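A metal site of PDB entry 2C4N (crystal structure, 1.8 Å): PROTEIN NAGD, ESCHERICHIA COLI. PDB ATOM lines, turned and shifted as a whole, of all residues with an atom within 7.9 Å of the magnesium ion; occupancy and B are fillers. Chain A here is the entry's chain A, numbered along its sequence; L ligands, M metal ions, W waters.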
ATOM      1  N   ASP A   9     -16.167  -5.723 -28.754  1.00  0.00           N
ATOM      2  CA  ASP A   9     -16.792  -5.334 -27.508  1.00  0.00           C
ATOM      3  C   ASP A   9     -15.718  -4.821 -26.548  1.00  0.00           C
ATOM      4  O   ASP A   9     -14.557  -5.224 -26.622  1.00  0.00           O
ATOM      5  CB  ASP A   9     -17.526  -6.520 -26.895  1.00  0.00           C
ATOM      6  CG  ASP A   9     -18.114  -6.184 -25.554  1.00  0.00           C
ATOM      7  OD1 ASP A   9     -18.931  -5.250 -25.487  1.00  0.00           O
ATOM      8  OD2 ASP A   9     -17.743  -6.862 -24.587  1.00  0.00           O
ATOM      9  N   ILE A  10     -16.101  -3.928 -25.639  1.00  0.00           N
ATOM     10  CA  ILE A  10     -15.151  -3.344 -24.701  1.00  0.00           C
ATOM     11  C   ILE A  10     -14.952  -4.076 -23.384  1.00  0.00           C
ATOM     12  O   ILE A  10     -13.895  -4.666 -23.138  1.00  0.00           O
ATOM     13  CB  ILE A  10     -15.511  -1.863 -24.423  1.00  0.00           C
ATOM     14  CG1 ILE A  10     -15.303  -1.040 -25.696  1.00  0.00           C
ATOM     15  CG2 ILE A  10     -14.680  -1.304 -23.264  1.00  0.00           C
ATOM     16  CD1 ILE A  10     -15.792   0.387 -25.618  1.00  0.00           C
ATOM     17  N   ASP A  11     -15.971  -4.041 -22.524  1.00  0.00           N
ATOM     18  CA  ASP A  11     -15.855  -4.677 -21.211  1.00  0.00           C
ATOM     19  C   ASP A  11     -15.727  -6.192 -21.220  1.00  0.00           C
ATOM     20  O   ASP A  11     -16.530  -6.891 -21.821  1.00  0.00           O
ATOM     21  CB  ASP A  11     -17.035  -4.219 -20.345  1.00  0.00           C
ATOM     22  CG  ASP A  11     -17.016  -2.720 -20.095  1.00  0.00           C
ATOM     23  OD1 ASP A  11     -16.039  -2.248 -19.491  1.00  0.00           O
ATOM     24  OD2 ASP A  11     -17.956  -2.022 -20.518  1.00  0.00           O
ATOM     25  N   GLY A  12     -14.713  -6.699 -20.536  1.00  0.00           N
ATOM     26  CA  GLY A  12     -14.484  -8.133 -20.488  1.00  0.00           C
ATOM     27  C   GLY A  12     -13.710  -8.637 -21.684  1.00  0.00           C
ATOM     28  O   GLY A  12     -13.428  -9.836 -21.797  1.00  0.00           O
ATOM     29  N   VAL A  13     -13.362  -7.725 -22.588  1.00  0.00           N
ATOM     30  CA  VAL A  13     -12.626  -8.061 -23.802  1.00  0.00           C
ATOM     31  C   VAL A  13     -11.350  -7.209 -23.915  1.00  0.00           C
ATOM     32  O   VAL A  13     -10.252  -7.736 -24.047  1.00  0.00           O
ATOM     33  CB  VAL A  13     -13.491  -7.816 -25.058  1.00  0.00           C
ATOM     34  CG1 VAL A  13     -12.690  -8.117 -26.319  1.00  0.00           C
ATOM     35  CG2 VAL A  13     -14.760  -8.673 -24.989  1.00  0.00           C
ATOM     36  N   LEU A  14     -11.527  -5.890 -23.865  1.00  0.00           N
ATOM     37  CA  LEU A  14     -10.399  -4.968 -23.979  1.00  0.00           C
ATOM     38  C   LEU A  14     -10.075  -4.342 -22.635  1.00  0.00           C
ATOM     39  O   LEU A  14      -8.920  -4.027 -22.344  1.00  0.00           O
ATOM     40  CB  LEU A  14     -10.742  -3.859 -24.991  1.00  0.00           C
ATOM     41  CG  LEU A  14     -10.988  -4.331 -26.430  1.00  0.00           C
ATOM     42  CD1 LEU A  14     -11.408  -3.161 -27.318  1.00  0.00           C
ATOM     43  CD2 LEU A  14      -9.723  -4.968 -26.978  1.00  0.00           C
ATOM     44  N   MET A  15     -11.099  -4.164 -21.838  1.00  0.00           N
ATOM     45  CA  MET A  15     -10.976  -3.597 -20.499  1.00  0.00           C
ATOM     46  C   MET A  15     -11.615  -4.437 -19.396  1.00  0.00           C
ATOM     47  O   MET A  15     -12.664  -4.952 -19.540  1.00  0.00           O
ATOM     48  CB  MET A  15     -11.566  -2.203 -20.453  1.00  0.00           C
ATOM     49  CG  MET A  15     -10.987  -1.266 -21.425  1.00  0.00           C
ATOM     50  SD  MET A  15      -9.335  -0.747 -21.129  1.00  0.00           S
ATOM     51  CE  MET A  15      -9.707   0.281 -19.965  1.00  0.00           C
ATOM     52  N   LEU A  41     -17.392  -1.290 -29.399  1.00  0.00           N
ATOM     53  CA  LEU A  41     -18.757  -1.253 -28.916  1.00  0.00           C
ATOM     54  C   LEU A  41     -18.984  -1.479 -27.435  1.00  0.00           C
ATOM     55  O   LEU A  41     -18.300  -2.282 -26.798  1.00  0.00           O
ATOM     56  CB  LEU A  41     -19.574  -2.286 -29.705  1.00  0.00           C
ATOM     57  CG  LEU A  41     -21.070  -2.433 -29.432  1.00  0.00           C
ATOM     58  CD1 LEU A  41     -21.809  -1.271 -30.097  1.00  0.00           C
ATOM     59  CD2 LEU A  41     -21.569  -3.763 -29.980  1.00  0.00           C
ATOM     60  N   THR A  42     -19.942  -0.739 -26.878  1.00  0.00           N
ATOM     61  CA  THR A  42     -20.313  -0.926 -25.488  1.00  0.00           C
ATOM     62  C   THR A  42     -21.804  -0.674 -25.352  1.00  0.00           C
ATOM     63  O   THR A  42     -22.349   0.247 -25.970  1.00  0.00           O
ATOM     64  CB  THR A  42     -19.571   0.001 -24.508  1.00  0.00           C
ATOM     65  OG1 THR A  42     -20.062  -0.234 -23.178  1.00  0.00           O
ATOM     66  CG2 THR A  42     -19.769   1.471 -24.863  1.00  0.00           C
ATOM     67  N   ASN A  43     -22.471  -1.503 -24.563  1.00  0.00           N
ATOM     68  CA  ASN A  43     -23.898  -1.385 -24.349  1.00  0.00           C
ATOM     69  C   ASN A  43     -24.269  -0.258 -23.412  1.00  0.00           C
ATOM     70  O   ASN A  43     -25.433   0.120 -23.333  1.00  0.00           O
ATOM     71  CB  ASN A  43     -24.448  -2.702 -23.801  1.00  0.00           C
ATOM     72  CG  ASN A  43     -25.470  -3.323 -24.708  1.00  0.00           C
ATOM     73  OD1 ASN A  43     -25.382  -3.191 -25.926  1.00  0.00           O
ATOM     74  ND2 ASN A  43     -26.440  -4.026 -24.120  1.00  0.00           N
ATOM     75  N   TYR A  44     -23.281   0.288 -22.699  1.00  0.00           N
ATOM     76  CA  TYR A  44     -23.577   1.354 -21.755  1.00  0.00           C
ATOM     77  C   TYR A  44     -23.551   2.723 -22.406  1.00  0.00           C
ATOM     78  O   TYR A  44     -22.711   3.034 -23.254  1.00  0.00           O
ATOM     79  CB  TYR A  44     -22.652   1.233 -20.540  1.00  0.00           C
ATOM     80  CG  TYR A  44     -22.963  -0.055 -19.767  1.00  0.00           C
ATOM     81  CD1 TYR A  44     -22.343  -1.261 -20.106  1.00  0.00           C
ATOM     82  CD2 TYR A  44     -23.952  -0.083 -18.784  1.00  0.00           C
ATOM     83  CE1 TYR A  44     -22.688  -2.463 -19.476  1.00  0.00           C
ATOM     84  CE2 TYR A  44     -24.307  -1.274 -18.146  1.00  0.00           C
ATOM     85  CZ  TYR A  44     -23.679  -2.455 -18.498  1.00  0.00           C
ATOM     86  OH  TYR A  44     -24.038  -3.639 -17.872  1.00  0.00           O
ATOM     87  N   LYS A 176     -27.290  -4.454 -27.531  1.00  0.00           N
ATOM     88  CA  LYS A 176     -27.230  -5.912 -27.592  1.00  0.00           C
ATOM     89  C   LYS A 176     -28.200  -6.453 -26.545  1.00  0.00           C
ATOM     90  O   LYS A 176     -28.377  -5.834 -25.495  1.00  0.00           O
ATOM     91  CB  LYS A 176     -25.813  -6.400 -27.268  1.00  0.00           C
ATOM     92  CG  LYS A 176     -24.725  -5.910 -28.208  1.00  0.00           C
ATOM     93  CD  LYS A 176     -23.341  -6.250 -27.652  1.00  0.00           C
ATOM     94  CE  LYS A 176     -22.990  -5.368 -26.443  1.00  0.00           C
ATOM     95  NZ  LYS A 176     -21.811  -5.891 -25.687  1.00  0.00           N
ATOM     96  N   VAL A 199     -16.083  -9.390 -31.906  1.00  0.00           N
ATOM     97  CA  VAL A 199     -15.375 -10.059 -30.815  1.00  0.00           C
ATOM     98  C   VAL A 199     -16.093  -9.670 -29.528  1.00  0.00           C
ATOM     99  O   VAL A 199     -16.323  -8.479 -29.278  1.00  0.00           O
ATOM    100  CB  VAL A 199     -13.900  -9.598 -30.724  1.00  0.00           C
ATOM    101  CG1 VAL A 199     -13.190 -10.328 -29.599  1.00  0.00           C
ATOM    102  CG2 VAL A 199     -13.186  -9.844 -32.049  1.00  0.00           C
ATOM    103  N   GLY A 200     -16.470 -10.655 -28.721  1.00  0.00           N
ATOM    104  CA  GLY A 200     -17.157 -10.345 -27.484  1.00  0.00           C
ATOM    105  C   GLY A 200     -16.949 -11.411 -26.423  1.00  0.00           C
ATOM    106  O   GLY A 200     -16.489 -12.514 -26.727  1.00  0.00           O
ATOM    107  N   ASP A 201     -17.318 -11.100 -25.183  1.00  0.00           N
ATOM    108  CA  ASP A 201     -17.157 -12.032 -24.083  1.00  0.00           C
ATOM    109  C   ASP A 201     -18.478 -12.603 -23.568  1.00  0.00           C
ATOM    110  O   ASP A 201     -18.470 -13.522 -22.749  1.00  0.00           O
ATOM    111  CB  ASP A 201     -16.446 -11.362 -22.910  1.00  0.00           C
ATOM    112  CG  ASP A 201     -17.267 -10.222 -22.327  1.00  0.00           C
ATOM    113  OD1 ASP A 201     -17.624  -9.331 -23.114  1.00  0.00           O
ATOM    114  OD2 ASP A 201     -17.537 -10.229 -21.105  1.00  0.00           O
ATOM    115  N   ASN A 202     -19.597 -12.063 -24.045  1.00  0.00           N
ATOM    116  CA  ASN A 202     -20.906 -12.530 -23.593  1.00  0.00           C
ATOM    117  C   ASN A 202     -21.685 -13.258 -24.689  1.00  0.00           C
ATOM    118  O   ASN A 202     -22.159 -12.645 -25.640  1.00  0.00           O
ATOM    119  CB  ASN A 202     -21.738 -11.356 -23.079  1.00  0.00           C
ATOM    120  CG  ASN A 202     -22.939 -11.809 -22.272  1.00  0.00           C
ATOM    121  OD1 ASN A 202     -23.468 -12.898 -22.492  1.00  0.00           O
ATOM    122  ND2 ASN A 202     -23.378 -10.977 -21.340  1.00  0.00           N
ATOM    123  N   THR A 205     -25.152 -11.841 -25.553  1.00  0.00           N
ATOM    124  CA  THR A 205     -25.296 -10.487 -26.072  1.00  0.00           C
ATOM    125  C   THR A 205     -24.433 -10.236 -27.316  1.00  0.00           C
ATOM    126  O   THR A 205     -24.951 -10.016 -28.402  1.00  0.00           O
ATOM    127  CB  THR A 205     -24.994  -9.435 -24.983  1.00  0.00           C
ATOM    128  OG1 THR A 205     -23.636  -9.556 -24.544  1.00  0.00           O
ATOM    129  CG2 THR A 205     -25.922  -9.637 -23.779  1.00  0.00           C
ATOM    130  N   ASP A 206     -23.116 -10.268 -27.155  1.00  0.00           N
ATOM    131  CA  ASP A 206     -22.228 -10.037 -28.293  1.00  0.00           C
ATOM    132  C   ASP A 206     -22.393 -11.117 -29.366  1.00  0.00           C
ATOM    133  O   ASP A 206     -22.595 -10.821 -30.541  1.00  0.00           O
ATOM    134  CB  ASP A 206     -20.760 -10.045 -27.856  1.00  0.00           C
ATOM    135  CG  ASP A 206     -20.474  -9.060 -26.757  1.00  0.00           C
ATOM    136  OD1 ASP A 206     -20.631  -7.849 -26.995  1.00  0.00           O
ATOM    137  OD2 ASP A 206     -20.087  -9.509 -25.650  1.00  0.00           O
ATOM    138  N   VAL A 220     -14.256 -14.486 -26.560  1.00  0.00           N
ATOM    139  CA  VAL A 220     -13.057 -14.534 -25.734  1.00  0.00           C
ATOM    140  C   VAL A 220     -13.554 -14.964 -24.372  1.00  0.00           C
ATOM    141  O   VAL A 220     -14.696 -14.690 -24.019  1.00  0.00           O
ATOM    142  CB  VAL A 220     -12.331 -13.158 -25.635  1.00  0.00           C
ATOM    143  CG1 VAL A 220     -11.647 -12.843 -26.947  1.00  0.00           C
ATOM    144  CG2 VAL A 220     -13.308 -12.052 -25.250  1.00  0.00           C
ATOM    145  N   GLY A 223     -14.059 -12.658 -20.042  1.00  0.00           N
ATOM    146  CA  GLY A 223     -15.150 -11.965 -19.387  1.00  0.00           C
ATOM    147  C   GLY A 223     -16.270 -12.821 -18.808  1.00  0.00           C
ATOM    148  O   GLY A 223     -16.030 -13.798 -18.102  1.00  0.00           O
ATOM    149  N   VAL A 224     -17.507 -12.435 -19.107  1.00  0.00           N
ATOM    150  CA  VAL A 224     -18.696 -13.113 -18.598  1.00  0.00           C
ATOM    151  C   VAL A 224     -18.843 -14.596 -18.922  1.00  0.00           C
ATOM    152  O   VAL A 224     -18.958 -15.420 -18.023  1.00  0.00           O
ATOM    153  CB  VAL A 224     -19.982 -12.397 -19.073  1.00  0.00           C
ATOM    154  CG1 VAL A 224     -21.215 -13.169 -18.602  1.00  0.00           C
ATOM    155  CG2 VAL A 224     -20.008 -10.976 -18.535  1.00  0.00           C
HETATM  156  P1  LIG L   1     -19.995  -3.943 -22.677  1.00  0.00           P
HETATM  157  O1  LIG L   1     -18.917  -3.159 -23.322  1.00  0.00           O
HETATM  158  O2  LIG L   1     -21.154  -4.047 -23.599  1.00  0.00           O
HETATM  159  O3  LIG L   1     -19.504  -5.293 -22.364  1.00  0.00           O
HETATM  160  O4  LIG L   1     -20.412  -3.270 -21.424  1.00  0.00           O
HETATM  161 MG    MG M   1     -18.566  -7.339 -22.573  1.00  0.00          MG
HETATM  162  O   HOH W   1     -20.450  -8.253 -23.563  1.00  0.00           O
HETATM  163  O   HOH W   2     -19.143  -8.066 -20.424  1.00  0.00           O
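The side-chain carboxylate (OD1) of Asp 9 is in salt-bridge range of the side-chain amino group (NZ) of Lys 176 (3.0 Å).
The backbone carbonyl oxygen (O) of Val 199 sits at hydrogen-bond distance from the backbone NH (N) of Asp 9 (2.8 Å).
OD2 of Asp 206 sits at hydrogen-bond distance from N of Asp 201, at 3.2 Å.
OD2 of Asp 201 is in hydrogen-bond range of N of Val 224.
Within 4 Å of the magnesium ion: Asp 9, Asp 11 and Asp 201.
The nearest printed residue that does not touch the magnesium ion is Asp 206 (4.1 Å).
The magnesium ion is bound by the backbone carbonyl oxygen (O) of Asp 11 (2.2 Å).
The magnesium ion is bound by OD2 of Asp 9 (2.2 Å).
The magnesium ion is bound by O3 of the ligand, at 2.3 Å.
OD1 of Asp 201 binds the magnesium ion, 2.3 Å away.
Water W1 is bound to the magnesium ion (2.3 Å).
Water W2 binds the magnesium ion, at 2.3 Å.
The magnesium ion has six donor atoms within binding distance.
Water W1 bridges the side-chain carboxylate of Asp 206 and the side-chain amino group of Lys 176.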
